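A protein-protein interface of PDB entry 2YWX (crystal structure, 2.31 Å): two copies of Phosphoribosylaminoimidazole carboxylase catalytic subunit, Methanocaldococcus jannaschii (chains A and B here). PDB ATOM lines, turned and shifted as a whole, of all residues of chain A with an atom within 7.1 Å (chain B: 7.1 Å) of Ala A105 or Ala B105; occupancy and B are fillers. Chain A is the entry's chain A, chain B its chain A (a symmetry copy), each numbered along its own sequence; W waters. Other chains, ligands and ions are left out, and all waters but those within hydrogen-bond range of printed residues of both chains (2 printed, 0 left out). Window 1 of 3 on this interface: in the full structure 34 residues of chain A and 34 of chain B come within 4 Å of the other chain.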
ATOM      1  N   PHE A  55     -22.902   0.926  20.584  1.00  0.00           N
ATOM      2  CA  PHE A  55     -23.834   0.111  21.359  1.00  0.00           C
ATOM      3  C   PHE A  55     -23.169  -0.374  22.655  1.00  0.00           C
ATOM      4  O   PHE A  55     -22.008  -0.807  22.649  1.00  0.00           O
ATOM      5  CB  PHE A  55     -24.275  -1.117  20.545  1.00  0.00           C
ATOM      6  CG  PHE A  55     -25.271  -0.814  19.451  1.00  0.00           C
ATOM      7  CD1 PHE A  55     -26.633  -0.783  19.721  1.00  0.00           C
ATOM      8  CD2 PHE A  55     -24.841  -0.559  18.149  1.00  0.00           C
ATOM      9  CE1 PHE A  55     -27.558  -0.506  18.707  1.00  0.00           C
ATOM     10  CE2 PHE A  55     -25.758  -0.280  17.131  1.00  0.00           C
ATOM     11  CZ  PHE A  55     -27.117  -0.254  17.413  1.00  0.00           C
ATOM     12  N   ALA A  57     -23.892  -3.104  25.501  1.00  0.00           N
ATOM     13  CA  ALA A  57     -24.719  -4.234  25.894  1.00  0.00           C
ATOM     14  C   ALA A  57     -24.312  -4.668  27.296  1.00  0.00           C
ATOM     15  O   ALA A  57     -23.130  -4.835  27.588  1.00  0.00           O
ATOM     16  CB  ALA A  57     -24.549  -5.380  24.902  1.00  0.00           C
ATOM     17  N   PRO A  66     -24.260  -9.203  24.145  1.00  0.00           N
ATOM     18  CA  PRO A  66     -23.216  -8.472  23.414  1.00  0.00           C
ATOM     19  C   PRO A  66     -22.950  -9.105  22.054  1.00  0.00           C
ATOM     20  O   PRO A  66     -22.918  -8.419  21.035  1.00  0.00           O
ATOM     21  CB  PRO A  66     -22.005  -8.566  24.338  1.00  0.00           C
ATOM     22  CG  PRO A  66     -22.634  -8.711  25.710  1.00  0.00           C
ATOM     23  CD  PRO A  66     -23.768  -9.657  25.456  1.00  0.00           C
ATOM     24  N   PRO A  76     -19.490  -0.245  16.669  1.00  0.00           N
ATOM     25  CA  PRO A  76     -18.768  -0.778  17.824  1.00  0.00           C
ATOM     26  C   PRO A  76     -19.756  -1.211  18.906  1.00  0.00           C
ATOM     27  O   PRO A  76     -20.688  -0.481  19.243  1.00  0.00           O
ATOM     28  CB  PRO A  76     -17.919   0.405  18.266  1.00  0.00           C
ATOM     29  CG  PRO A  76     -17.652   1.121  16.983  1.00  0.00           C
ATOM     30  CD  PRO A  76     -19.000   1.102  16.327  1.00  0.00           C
ATOM     31  N   VAL A  77     -19.558  -2.410  19.435  1.00  0.00           N
ATOM     32  CA  VAL A  77     -20.425  -2.923  20.484  1.00  0.00           C
ATOM     33  C   VAL A  77     -19.576  -3.161  21.731  1.00  0.00           C
ATOM     34  O   VAL A  77     -18.631  -3.944  21.708  1.00  0.00           O
ATOM     35  CB  VAL A  77     -21.123  -4.245  20.049  1.00  0.00           C
ATOM     36  CG1 VAL A  77     -21.951  -4.804  21.200  1.00  0.00           C
ATOM     37  CG2 VAL A  77     -22.033  -3.988  18.858  1.00  0.00           C
ATOM     38  N   ILE A  78     -19.901  -2.452  22.809  1.00  0.00           N
ATOM     39  CA  ILE A  78     -19.172  -2.594  24.066  1.00  0.00           C
ATOM     40  C   ILE A  78     -19.988  -3.487  24.989  1.00  0.00           C
ATOM     41  O   ILE A  78     -21.187  -3.268  25.161  1.00  0.00           O
ATOM     42  CB  ILE A  78     -18.975  -1.230  24.761  1.00  0.00           C
ATOM     43  CG1 ILE A  78     -18.127  -0.311  23.869  1.00  0.00           C
ATOM     44  CG2 ILE A  78     -18.337  -1.433  26.147  1.00  0.00           C
ATOM     45  CD1 ILE A  78     -18.329   1.180  24.146  1.00  0.00           C
ATOM     46  N   ALA A  79     -19.340  -4.490  25.572  1.00  0.00           N
ATOM     47  CA  ALA A  79     -20.012  -5.408  26.480  1.00  0.00           C
ATOM     48  C   ALA A  79     -19.595  -5.152  27.917  1.00  0.00           C
ATOM     49  O   ALA A  79     -18.429  -4.858  28.202  1.00  0.00           O
ATOM     50  CB  ALA A  79     -19.693  -6.850  26.109  1.00  0.00           C
ATOM     51  N   VAL A  80     -20.564  -5.254  28.819  1.00  0.00           N
ATOM     52  CA  VAL A  80     -20.299  -5.083  30.240  1.00  0.00           C
ATOM     53  C   VAL A  80     -20.737  -6.365  30.919  1.00  0.00           C
ATOM     54  O   VAL A  80     -21.930  -6.626  31.043  1.00  0.00           O
ATOM     55  CB  VAL A  80     -21.096  -3.905  30.849  1.00  0.00           C
ATOM     56  CG1 VAL A  80     -20.789  -3.793  32.345  1.00  0.00           C
ATOM     57  CG2 VAL A  80     -20.733  -2.609  30.142  1.00  0.00           C
ATOM     58  N   SER A  95     -18.555 -13.118  26.581  1.00  0.00           N
ATOM     59  CA  SER A  95     -18.641 -11.957  25.701  1.00  0.00           C
ATOM     60  C   SER A  95     -17.294 -11.555  25.101  1.00  0.00           C
ATOM     61  O   SER A  95     -17.243 -11.054  23.978  1.00  0.00           O
ATOM     62  CB  SER A  95     -19.269 -10.768  26.441  1.00  0.00           C
ATOM     63  OG  SER A  95     -18.539 -10.431  27.606  1.00  0.00           O
ATOM     64  N   VAL A  96     -16.207 -11.792  25.833  1.00  0.00           N
ATOM     65  CA  VAL A  96     -14.871 -11.434  25.353  1.00  0.00           C
ATOM     66  C   VAL A  96     -14.308 -12.400  24.306  1.00  0.00           C
ATOM     67  O   VAL A  96     -13.649 -11.980  23.353  1.00  0.00           O
ATOM     68  CB  VAL A  96     -13.847 -11.341  26.522  1.00  0.00           C
ATOM     69  CG1 VAL A  96     -13.644 -12.709  27.156  1.00  0.00           C
ATOM     70  CG2 VAL A  96     -12.521 -10.792  26.015  1.00  0.00           C
ATOM     71  N   MET A  98     -15.158 -13.727  21.611  1.00  0.00           N
ATOM     72  CA  MET A  98     -15.890 -13.768  20.351  1.00  0.00           C
ATOM     73  C   MET A  98     -15.007 -14.412  19.300  1.00  0.00           C
ATOM     74  O   MET A  98     -13.790 -14.489  19.466  1.00  0.00           O
ATOM     75  CB  MET A  98     -16.284 -12.357  19.907  1.00  0.00           C
ATOM     76  CG  MET A  98     -17.507 -11.805  20.622  1.00  0.00           C
ATOM     77  SD  MET A  98     -19.013 -12.765  20.284  1.00  0.00           S
ATOM     78  CE  MET A  98     -19.595 -11.991  18.778  1.00  0.00           C
ATOM     79  N   PRO A 103     -16.007  -8.868  16.320  1.00  0.00           N
ATOM     80  CA  PRO A 103     -15.492  -8.466  17.630  1.00  0.00           C
ATOM     81  C   PRO A 103     -16.460  -7.704  18.542  1.00  0.00           C
ATOM     82  O   PRO A 103     -17.449  -7.108  18.096  1.00  0.00           O
ATOM     83  CB  PRO A 103     -14.285  -7.615  17.266  1.00  0.00           C
ATOM     84  CG  PRO A 103     -14.774  -6.905  16.039  1.00  0.00           C
ATOM     85  CD  PRO A 103     -15.419  -8.040  15.251  1.00  0.00           C
ATOM     86  N   VAL A 104     -16.136  -7.728  19.830  1.00  0.00           N
ATOM     87  CA  VAL A 104     -16.899  -7.029  20.860  1.00  0.00           C
ATOM     88  C   VAL A 104     -15.890  -6.407  21.827  1.00  0.00           C
ATOM     89  O   VAL A 104     -15.000  -7.096  22.328  1.00  0.00           O
ATOM     90  CB  VAL A 104     -17.830  -8.001  21.649  1.00  0.00           C
ATOM     91  CG1 VAL A 104     -18.155  -7.427  23.016  1.00  0.00           C
ATOM     92  CG2 VAL A 104     -19.132  -8.221  20.875  1.00  0.00           C
ATOM     93  N   ALA A 105     -16.014  -5.107  22.068  1.00  0.00           N
ATOM     94  CA  ALA A 105     -15.120  -4.420  22.997  1.00  0.00           C
ATOM     95  C   ALA A 105     -15.596  -4.743  24.412  1.00  0.00           C
ATOM     96  O   ALA A 105     -16.705  -4.374  24.810  1.00  0.00           O
ATOM     97  CB  ALA A 105     -15.156  -2.905  22.760  1.00  0.00           C
ATOM     98  N   THR A 106     -14.756  -5.424  25.173  1.00  0.00           N
ATOM     99  CA  THR A 106     -15.120  -5.803  26.532  1.00  0.00           C
ATOM    100  C   THR A 106     -14.409  -4.972  27.598  1.00  0.00           C
ATOM    101  O   THR A 106     -13.209  -4.679  27.482  1.00  0.00           O
ATOM    102  CB  THR A 106     -14.797  -7.288  26.769  1.00  0.00           C
ATOM    103  OG1 THR A 106     -15.503  -8.078  25.803  1.00  0.00           O
ATOM    104  CG2 THR A 106     -15.196  -7.723  28.183  1.00  0.00           C
ATOM    105  N   VAL A 107     -15.160  -4.577  28.623  1.00  0.00           N
ATOM    106  CA  VAL A 107     -14.590  -3.831  29.737  1.00  0.00           C
ATOM    107  C   VAL A 107     -14.789  -4.706  30.962  1.00  0.00           C
ATOM    108  O   VAL A 107     -15.449  -5.742  30.877  1.00  0.00           O
ATOM    109  CB  VAL A 107     -15.273  -2.451  29.957  1.00  0.00           C
ATOM    110  CG1 VAL A 107     -14.994  -1.541  28.780  1.00  0.00           C
ATOM    111  CG2 VAL A 107     -16.761  -2.617  30.157  1.00  0.00           C
ATOM    112  N   LEU A 118     -15.651   4.688  27.356  1.00  0.00           N
ATOM    113  CA  LEU A 118     -15.123   4.102  26.131  1.00  0.00           C
ATOM    114  C   LEU A 118     -15.941   4.561  24.938  1.00  0.00           C
ATOM    115  O   LEU A 118     -15.392   4.899  23.884  1.00  0.00           O
ATOM    116  CB  LEU A 118     -15.128   2.566  26.215  1.00  0.00           C
ATOM    117  CG  LEU A 118     -14.658   1.813  24.962  1.00  0.00           C
ATOM    118  CD1 LEU A 118     -13.279   2.299  24.526  1.00  0.00           C
ATOM    119  CD2 LEU A 118     -14.617   0.334  25.253  1.00  0.00           C
ATOM    120  N   GLU A 121     -15.123   8.141  24.117  1.00  0.00           N
ATOM    121  CA  GLU A 121     -13.818   8.254  23.469  1.00  0.00           C
ATOM    122  C   GLU A 121     -13.985   7.951  21.979  1.00  0.00           C
ATOM    123  O   GLU A 121     -13.291   8.518  21.139  1.00  0.00           O
ATOM    124  CB  GLU A 121     -12.807   7.268  24.087  1.00  0.00           C
ATOM    125  CG  GLU A 121     -12.628   7.391  25.603  1.00  0.00           C
ATOM    126  CD  GLU A 121     -11.501   6.512  26.137  1.00  0.00           C
ATOM    127  OE1 GLU A 121     -11.243   5.439  25.552  1.00  0.00           O
ATOM    128  OE2 GLU A 121     -10.882   6.883  27.156  1.00  0.00           O
ATOM    129  N   ILE A 122     -14.907   7.050  21.657  1.00  0.00           N
ATOM    130  CA  ILE A 122     -15.152   6.702  20.260  1.00  0.00           C
ATOM    131  C   ILE A 122     -15.844   7.884  19.575  1.00  0.00           C
ATOM    132  O   ILE A 122     -15.440   8.309  18.486  1.00  0.00           O
ATOM    133  CB  ILE A 122     -16.030   5.418  20.140  1.00  0.00           C
ATOM    134  CG1 ILE A 122     -15.257   4.202  20.658  1.00  0.00           C
ATOM    135  CG2 ILE A 122     -16.436   5.186  18.700  1.00  0.00           C
ATOM    136  CD1 ILE A 122     -16.093   2.936  20.791  1.00  0.00           C
ATOM    137  N   PHE B  55      -5.627   2.954  19.013  1.00  0.00           N
ATOM    138  CA  PHE B  55      -4.410   2.260  19.426  1.00  0.00           C
ATOM    139  C   PHE B  55      -4.702   0.775  19.682  1.00  0.00           C
ATOM    140  O   PHE B  55      -5.715   0.426  20.304  1.00  0.00           O
ATOM    141  CB  PHE B  55      -3.854   2.881  20.719  1.00  0.00           C
ATOM    142  CG  PHE B  55      -3.167   4.211  20.526  1.00  0.00           C
ATOM    143  CD1 PHE B  55      -1.822   4.272  20.184  1.00  0.00           C
ATOM    144  CD2 PHE B  55      -3.870   5.405  20.688  1.00  0.00           C
ATOM    145  CE1 PHE B  55      -1.183   5.505  20.009  1.00  0.00           C
ATOM    146  CE2 PHE B  55      -3.239   6.641  20.512  1.00  0.00           C
ATOM    147  CZ  PHE B  55      -1.895   6.688  20.173  1.00  0.00           C
ATOM    148  N   ALA B  57      -2.876  -2.334  21.435  1.00  0.00           N
ATOM    149  CA  ALA B  57      -1.756  -2.753  22.263  1.00  0.00           C
ATOM    150  C   ALA B  57      -1.794  -4.270  22.397  1.00  0.00           C
ATOM    151  O   ALA B  57      -2.835  -4.852  22.695  1.00  0.00           O
ATOM    152  CB  ALA B  57      -1.835  -2.086  23.632  1.00  0.00           C
ATOM    153  N   PRO B  66      -1.375  -2.226  27.510  1.00  0.00           N
ATOM    154  CA  PRO B  66      -2.672  -1.617  27.186  1.00  0.00           C
ATOM    155  C   PRO B  66      -3.026  -0.516  28.177  1.00  0.00           C
ATOM    156  O   PRO B  66      -3.398   0.589  27.786  1.00  0.00           O
ATOM    157  CB  PRO B  66      -3.643  -2.793  27.262  1.00  0.00           C
ATOM    158  CG  PRO B  66      -2.761  -3.984  26.942  1.00  0.00           C
ATOM    159  CD  PRO B  66      -1.506  -3.680  27.702  1.00  0.00           C
ATOM    160  N   PRO B  76      -9.328   5.656  21.722  1.00  0.00           N
ATOM    161  CA  PRO B  76      -9.690   4.282  22.069  1.00  0.00           C
ATOM    162  C   PRO B  76      -8.451   3.388  22.032  1.00  0.00           C
ATOM    163  O   PRO B  76      -7.666   3.432  21.086  1.00  0.00           O
ATOM    164  CB  PRO B  76     -10.693   3.913  20.986  1.00  0.00           C
ATOM    165  CG  PRO B  76     -11.343   5.221  20.675  1.00  0.00           C
ATOM    166  CD  PRO B  76     -10.166   6.149  20.615  1.00  0.00           C
ATOM    167  N   VAL B  77      -8.272   2.591  23.075  1.00  0.00           N
ATOM    168  CA  VAL B  77      -7.136   1.684  23.145  1.00  0.00           C
ATOM    169  C   VAL B  77      -7.670   0.255  23.211  1.00  0.00           C
ATOM    170  O   VAL B  77      -8.400  -0.101  24.131  1.00  0.00           O
ATOM    171  CB  VAL B  77      -6.245   1.984  24.386  1.00  0.00           C
ATOM    172  CG1 VAL B  77      -5.118   0.962  24.479  1.00  0.00           C
ATOM    173  CG2 VAL B  77      -5.647   3.377  24.277  1.00  0.00           C
ATOM    174  N   ILE B  78      -7.327  -0.549  22.207  1.00  0.00           N
ATOM    175  CA  ILE B  78      -7.767  -1.941  22.159  1.00  0.00           C
ATOM    176  C   ILE B  78      -6.615  -2.817  22.629  1.00  0.00           C
ATOM    177  O   ILE B  78      -5.487  -2.661  22.162  1.00  0.00           O
ATOM    178  CB  ILE B  78      -8.141  -2.363  20.722  1.00  0.00           C
ATOM    179  CG1 ILE B  78      -9.323  -1.518  20.225  1.00  0.00           C
ATOM    180  CG2 ILE B  78      -8.456  -3.869  20.683  1.00  0.00           C
ATOM    181  CD1 ILE B  78      -9.420  -1.425  18.700  1.00  0.00           C
ATOM    182  N   ALA B  79      -6.902  -3.728  23.554  1.00  0.00           N
ATOM    183  CA  ALA B  79      -5.886  -4.629  24.078  1.00  0.00           C
ATOM    184  C   ALA B  79      -6.085  -6.038  23.550  1.00  0.00           C
ATOM    185  O   ALA B  79      -7.216  -6.514  23.408  1.00  0.00           O
ATOM    186  CB  ALA B  79      -5.928  -4.649  25.601  1.00  0.00           C
ATOM    187  N   VAL B  80      -4.973  -6.696  23.246  1.00  0.00           N
ATOM    188  CA  VAL B  80      -5.009  -8.073  22.775  1.00  0.00           C
ATOM    189  C   VAL B  80      -4.175  -8.884  23.745  1.00  0.00           C
ATOM    190  O   VAL B  80      -2.952  -8.785  23.748  1.00  0.00           O
ATOM    191  CB  VAL B  80      -4.407  -8.225  21.358  1.00  0.00           C
ATOM    192  CG1 VAL B  80      -4.457  -9.695  20.932  1.00  0.00           C
ATOM    193  CG2 VAL B  80      -5.177  -7.367  20.368  1.00  0.00           C
ATOM    194  N   SER B  95      -5.502  -6.658  31.649  1.00  0.00           N
ATOM    195  CA  SER B  95      -5.843  -5.561  30.750  1.00  0.00           C
ATOM    196  C   SER B  95      -7.332  -5.214  30.760  1.00  0.00           C
ATOM    197  O   SER B  95      -7.697  -4.054  30.574  1.00  0.00           O
ATOM    198  CB  SER B  95      -5.380  -5.875  29.321  1.00  0.00           C
ATOM    199  OG  SER B  95      -5.946  -7.079  28.839  1.00  0.00           O
ATOM    200  N   VAL B  96      -8.186  -6.208  30.998  1.00  0.00           N
ATOM    201  CA  VAL B  96      -9.632  -5.982  31.018  1.00  0.00           C
ATOM    202  C   VAL B  96     -10.138  -5.315  32.300  1.00  0.00           C
ATOM    203  O   VAL B  96     -11.037  -4.472  32.258  1.00  0.00           O
ATOM    204  CB  VAL B  96     -10.423  -7.308  30.820  1.00  0.00           C
ATOM    205  CG1 VAL B  96     -10.191  -8.242  31.999  1.00  0.00           C
ATOM    206  CG2 VAL B  96     -11.909  -7.015  30.664  1.00  0.00           C
ATOM    207  N   MET B  98      -9.507  -2.834  34.086  1.00  0.00           N
ATOM    208  CA  MET B  98      -9.024  -1.476  34.309  1.00  0.00           C
ATOM    209  C   MET B  98      -9.911  -0.812  35.344  1.00  0.00           C
ATOM    210  O   MET B  98     -11.028  -1.264  35.594  1.00  0.00           O
ATOM    211  CB  MET B  98      -9.049  -0.671  33.008  1.00  0.00           C
ATOM    212  CG  MET B  98      -7.875  -0.957  32.083  1.00  0.00           C
ATOM    213  SD  MET B  98      -6.277  -0.492  32.810  1.00  0.00           S
ATOM    214  CE  MET B  98      -6.167   1.235  32.347  1.00  0.00           C
ATOM    215  N   PRO B 103     -10.755   3.402  30.638  1.00  0.00           N
ATOM    216  CA  PRO B 103     -11.104   2.122  30.020  1.00  0.00           C
ATOM    217  C   PRO B 103     -10.188   1.634  28.892  1.00  0.00           C
ATOM    218  O   PRO B 103      -9.458   2.407  28.260  1.00  0.00           O
ATOM    219  CB  PRO B 103     -12.518   2.370  29.518  1.00  0.00           C
ATOM    220  CG  PRO B 103     -12.433   3.795  29.063  1.00  0.00           C
ATOM    221  CD  PRO B 103     -11.699   4.457  30.224  1.00  0.00           C
ATOM    222  N   VAL B 104     -10.261   0.330  28.650  1.00  0.00           N
ATOM    223  CA  VAL B 104      -9.505  -0.330  27.589  1.00  0.00           C
ATOM    224  C   VAL B 104     -10.439  -1.352  26.937  1.00  0.00           C
ATOM    225  O   VAL B 104     -11.043  -2.174  27.627  1.00  0.00           O
ATOM    226  CB  VAL B 104      -8.250  -1.070  28.149  1.00  0.00           C
ATOM    227  CG1 VAL B 104      -7.825  -2.177  27.202  1.00  0.00           C
ATOM    228  CG2 VAL B 104      -7.094  -0.083  28.319  1.00  0.00           C
ATOM    229  N   ALA B 105     -10.574  -1.282  25.618  1.00  0.00           N
ATOM    230  CA  ALA B 105     -11.419  -2.227  24.892  1.00  0.00           C
ATOM    231  C   ALA B 105     -10.636  -3.532  24.759  1.00  0.00           C
ATOM    232  O   ALA B 105      -9.587  -3.581  24.109  1.00  0.00           O
ATOM    233  CB  ALA B 105     -11.772  -1.679  23.504  1.00  0.00           C
ATOM    234  N   THR B 106     -11.147  -4.589  25.367  1.00  0.00           N
ATOM    235  CA  THR B 106     -10.468  -5.878  25.321  1.00  0.00           C
ATOM    236  C   THR B 106     -11.145  -6.881  24.391  1.00  0.00           C
ATOM    237  O   THR B 106     -12.382  -6.984  24.357  1.00  0.00           O
ATOM    238  CB  THR B 106     -10.395  -6.485  26.732  1.00  0.00           C
ATOM    239  OG1 THR B 106      -9.712  -5.569  27.599  1.00  0.00           O
ATOM    240  CG2 THR B 106      -9.659  -7.829  26.720  1.00  0.00           C
ATOM    241  N   VAL B 107     -10.333  -7.603  23.623  1.00  0.00           N
ATOM    242  CA  VAL B 107     -10.849  -8.638  22.737  1.00  0.00           C
ATOM    243  C   VAL B 107     -10.238  -9.939  23.226  1.00  0.00           C
ATOM    244  O   VAL B 107      -9.385  -9.922  24.114  1.00  0.00           O
ATOM    245  CB  VAL B 107     -10.470  -8.404  21.246  1.00  0.00           C
ATOM    246  CG1 VAL B 107     -11.157  -7.159  20.726  1.00  0.00           C
ATOM    247  CG2 VAL B 107      -8.973  -8.289  21.086  1.00  0.00           C
ATOM    248  N   LEU B 118     -12.206  -4.362  15.040  1.00  0.00           N
ATOM    249  CA  LEU B 118     -12.798  -3.439  15.999  1.00  0.00           C
ATOM    250  C   LEU B 118     -12.334  -2.021  15.715  1.00  0.00           C
ATOM    251  O   LEU B 118     -13.126  -1.074  15.757  1.00  0.00           O
ATOM    252  CB  LEU B 118     -12.427  -3.836  17.438  1.00  0.00           C
ATOM    253  CG  LEU B 118     -12.931  -2.908  18.554  1.00  0.00           C
ATOM    254  CD1 LEU B 118     -14.440  -2.708  18.449  1.00  0.00           C
ATOM    255  CD2 LEU B 118     -12.579  -3.501  19.895  1.00  0.00           C
ATOM    256  N   GLU B 121     -14.082  -0.684  12.663  1.00  0.00           N
ATOM    257  CA  GLU B 121     -15.473  -0.342  12.952  1.00  0.00           C
ATOM    258  C   GLU B 121     -15.512   1.050  13.584  1.00  0.00           C
ATOM    259  O   GLU B 121     -16.456   1.809  13.380  1.00  0.00           O
ATOM    260  CB  GLU B 121     -16.104  -1.365  13.917  1.00  0.00           C
ATOM    261  CG  GLU B 121     -16.031  -2.823  13.452  1.00  0.00           C
ATOM    262  CD  GLU B 121     -16.813  -3.771  14.357  1.00  0.00           C
ATOM    263  OE1 GLU B 121     -16.920  -3.496  15.571  1.00  0.00           O
ATOM    264  OE2 GLU B 121     -17.306  -4.804  13.860  1.00  0.00           O
ATOM    265  N   ILE B 122     -14.482   1.380  14.357  1.00  0.00           N
ATOM    266  CA  ILE B 122     -14.420   2.692  14.993  1.00  0.00           C
ATOM    267  C   ILE B 122     -14.151   3.747  13.917  1.00  0.00           C
ATOM    268  O   ILE B 122     -14.830   4.780  13.858  1.00  0.00           O
ATOM    269  CB  ILE B 122     -13.308   2.741  16.087  1.00  0.00           C
ATOM    270  CG1 ILE B 122     -13.677   1.819  17.253  1.00  0.00           C
ATOM    271  CG2 ILE B 122     -13.125   4.155  16.596  1.00  0.00           C
ATOM    272  CD1 ILE B 122     -12.564   1.621  18.274  1.00  0.00           C
HETATM  273  O   HOH W   1      -9.111   5.078  28.287  1.00  0.00           O
HETATM  274  O   HOH W   2     -18.386  -6.659  15.611  1.00  0.00           O
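Water W2 bridges the backbone carbonyl oxygen of Pro A103 (2.7 Å) and the side-chain carboxylate of Glu B121 (2.8 Å).
Water W1 bridges the backbone carbonyl oxygen (O) of Pro B103 (2.7 Å) and the side-chain carboxylate (OE2) of Glu A121 (2.8 Å).
Of chain B, only Ala B105, Thr B106 and Leu B118 come within 4 Å of Ala A105.
Of chain A, only Ala A105, Thr A106 and Leu A118 come within 4 Å of Ala B105.
Of the printed residues of chain B, Glu A121 touches Pro B76 and Pro B103.
Printed residues of chain B within 4 Å of Leu A118: Pro B103 (3.8 Å) and Ala B105 (3.9 Å).
Printed residues of chain A within 4 Å of Thr B106: Val A104 (3.3 Å), Ala A105 (3.9 Å) and Thr A106 (3.0 Å).
Ala A57 touches none of the printed residues of chain B.
The nearest residue of chain B that does not touch Ala A105 is Val B107 (5.3 Å).
The nearest residue of chain A that does not touch Ala B105 is Val A107 (5.3 Å).
Printed residues of chain A that touch a printed residue of chain B: Pro A76, Val A96, Pro A103, Val A104, Ala A105, Thr A106, Val A107, Leu A118 and Glu A121.
Hydrophobic or aromatic side chains of chain A that line the printed part of chain B: Pro A76, Val A96, Pro A103, Ala A105 and Leu A118.
Among the printed residues, 16 pairs touch across the chains.
Among the printed residues, no Asp or Glu carboxylate lies within 4 Å of a Lys or Arg side-chain nitrogen of the other chain.
Pro A76 touches Glu B121, and with the chains exchanged Glu A121 touches Pro B76.
Pro A103 touches Leu B118, and with the chains exchanged Leu A118 touches Pro B103.
Ala B105 touches its own counterpart, Ala A105.
Ala A105 touches Thr B106, and with the chains exchanged Thr A106 touches Ala B105.
Positions printed for both chains: 55, 57, 66, 76, 77, 78, 79, 80, 95, 96, 98, 103, 104, 105, 106, 107, 118, 121 and 122.
Of the 16 pairs that touch across the chains among the printed residues, 16 have their exchanged pair printed and touching as well.
N of Thr A106 sits at hydrogen-bond distance from O of Thr B106, at 3.0 Å.
The backbone carbonyl oxygen of Thr A106 lies close to the backbone carbonyl oxygen of Val B104 (3.3 Å).
O of Thr B106 lies close to O of Val A104 (3.3 Å).
The backbone carbonyl oxygen (O) of Ala A79 lies within hydrogen-bond range of the backbone NH (N) of Val A107 (3.3 Å).
O of Pro B76 is in hydrogen-bond range of N of Phe B55, 2.9 Å away.
The backbone carbonyl oxygen of Ala A105 is in hydrogen-bond range of the backbone NH of Ala A79 (2.7 Å).
The backbone NH (N) of Ala B105 sits at hydrogen-bond distance from the backbone carbonyl oxygen (O) of Val B77 (2.9 Å).
The backbone carbonyl oxygen of Ala B105 sits at hydrogen-bond distance from the backbone NH of Ala B79 (2.7 Å).
The backbone carbonyl oxygen of Ala B79 sits at hydrogen-bond distance from the backbone NH of Val B107 (3.3 Å).
Among the printed residues, pairs that only touch across the chains: Ala A105 with Ala B105 (3.7 Å), Val A107 with Val B96 (3.7 Å), Val A96 with Val B107 (3.7 Å), Pro A103 with Leu B118 (3.7 Å), Leu A118 with Pro B103 (3.8 Å), Glu A121 with Pro B76 (3.9 Å), Pro A76 with Glu B121 (3.9 Å), Ala A105 with Leu B118 (3.9 Å), Leu A118 with Ala B105 (3.9 Å), Thr A106 with Ala B105 (3.9 Å), Ala A105 with Thr B106 (3.9 Å), Pro A103 with Glu B121 (3.9 Å) and Glu A121 with Pro B103 (3.9 Å).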
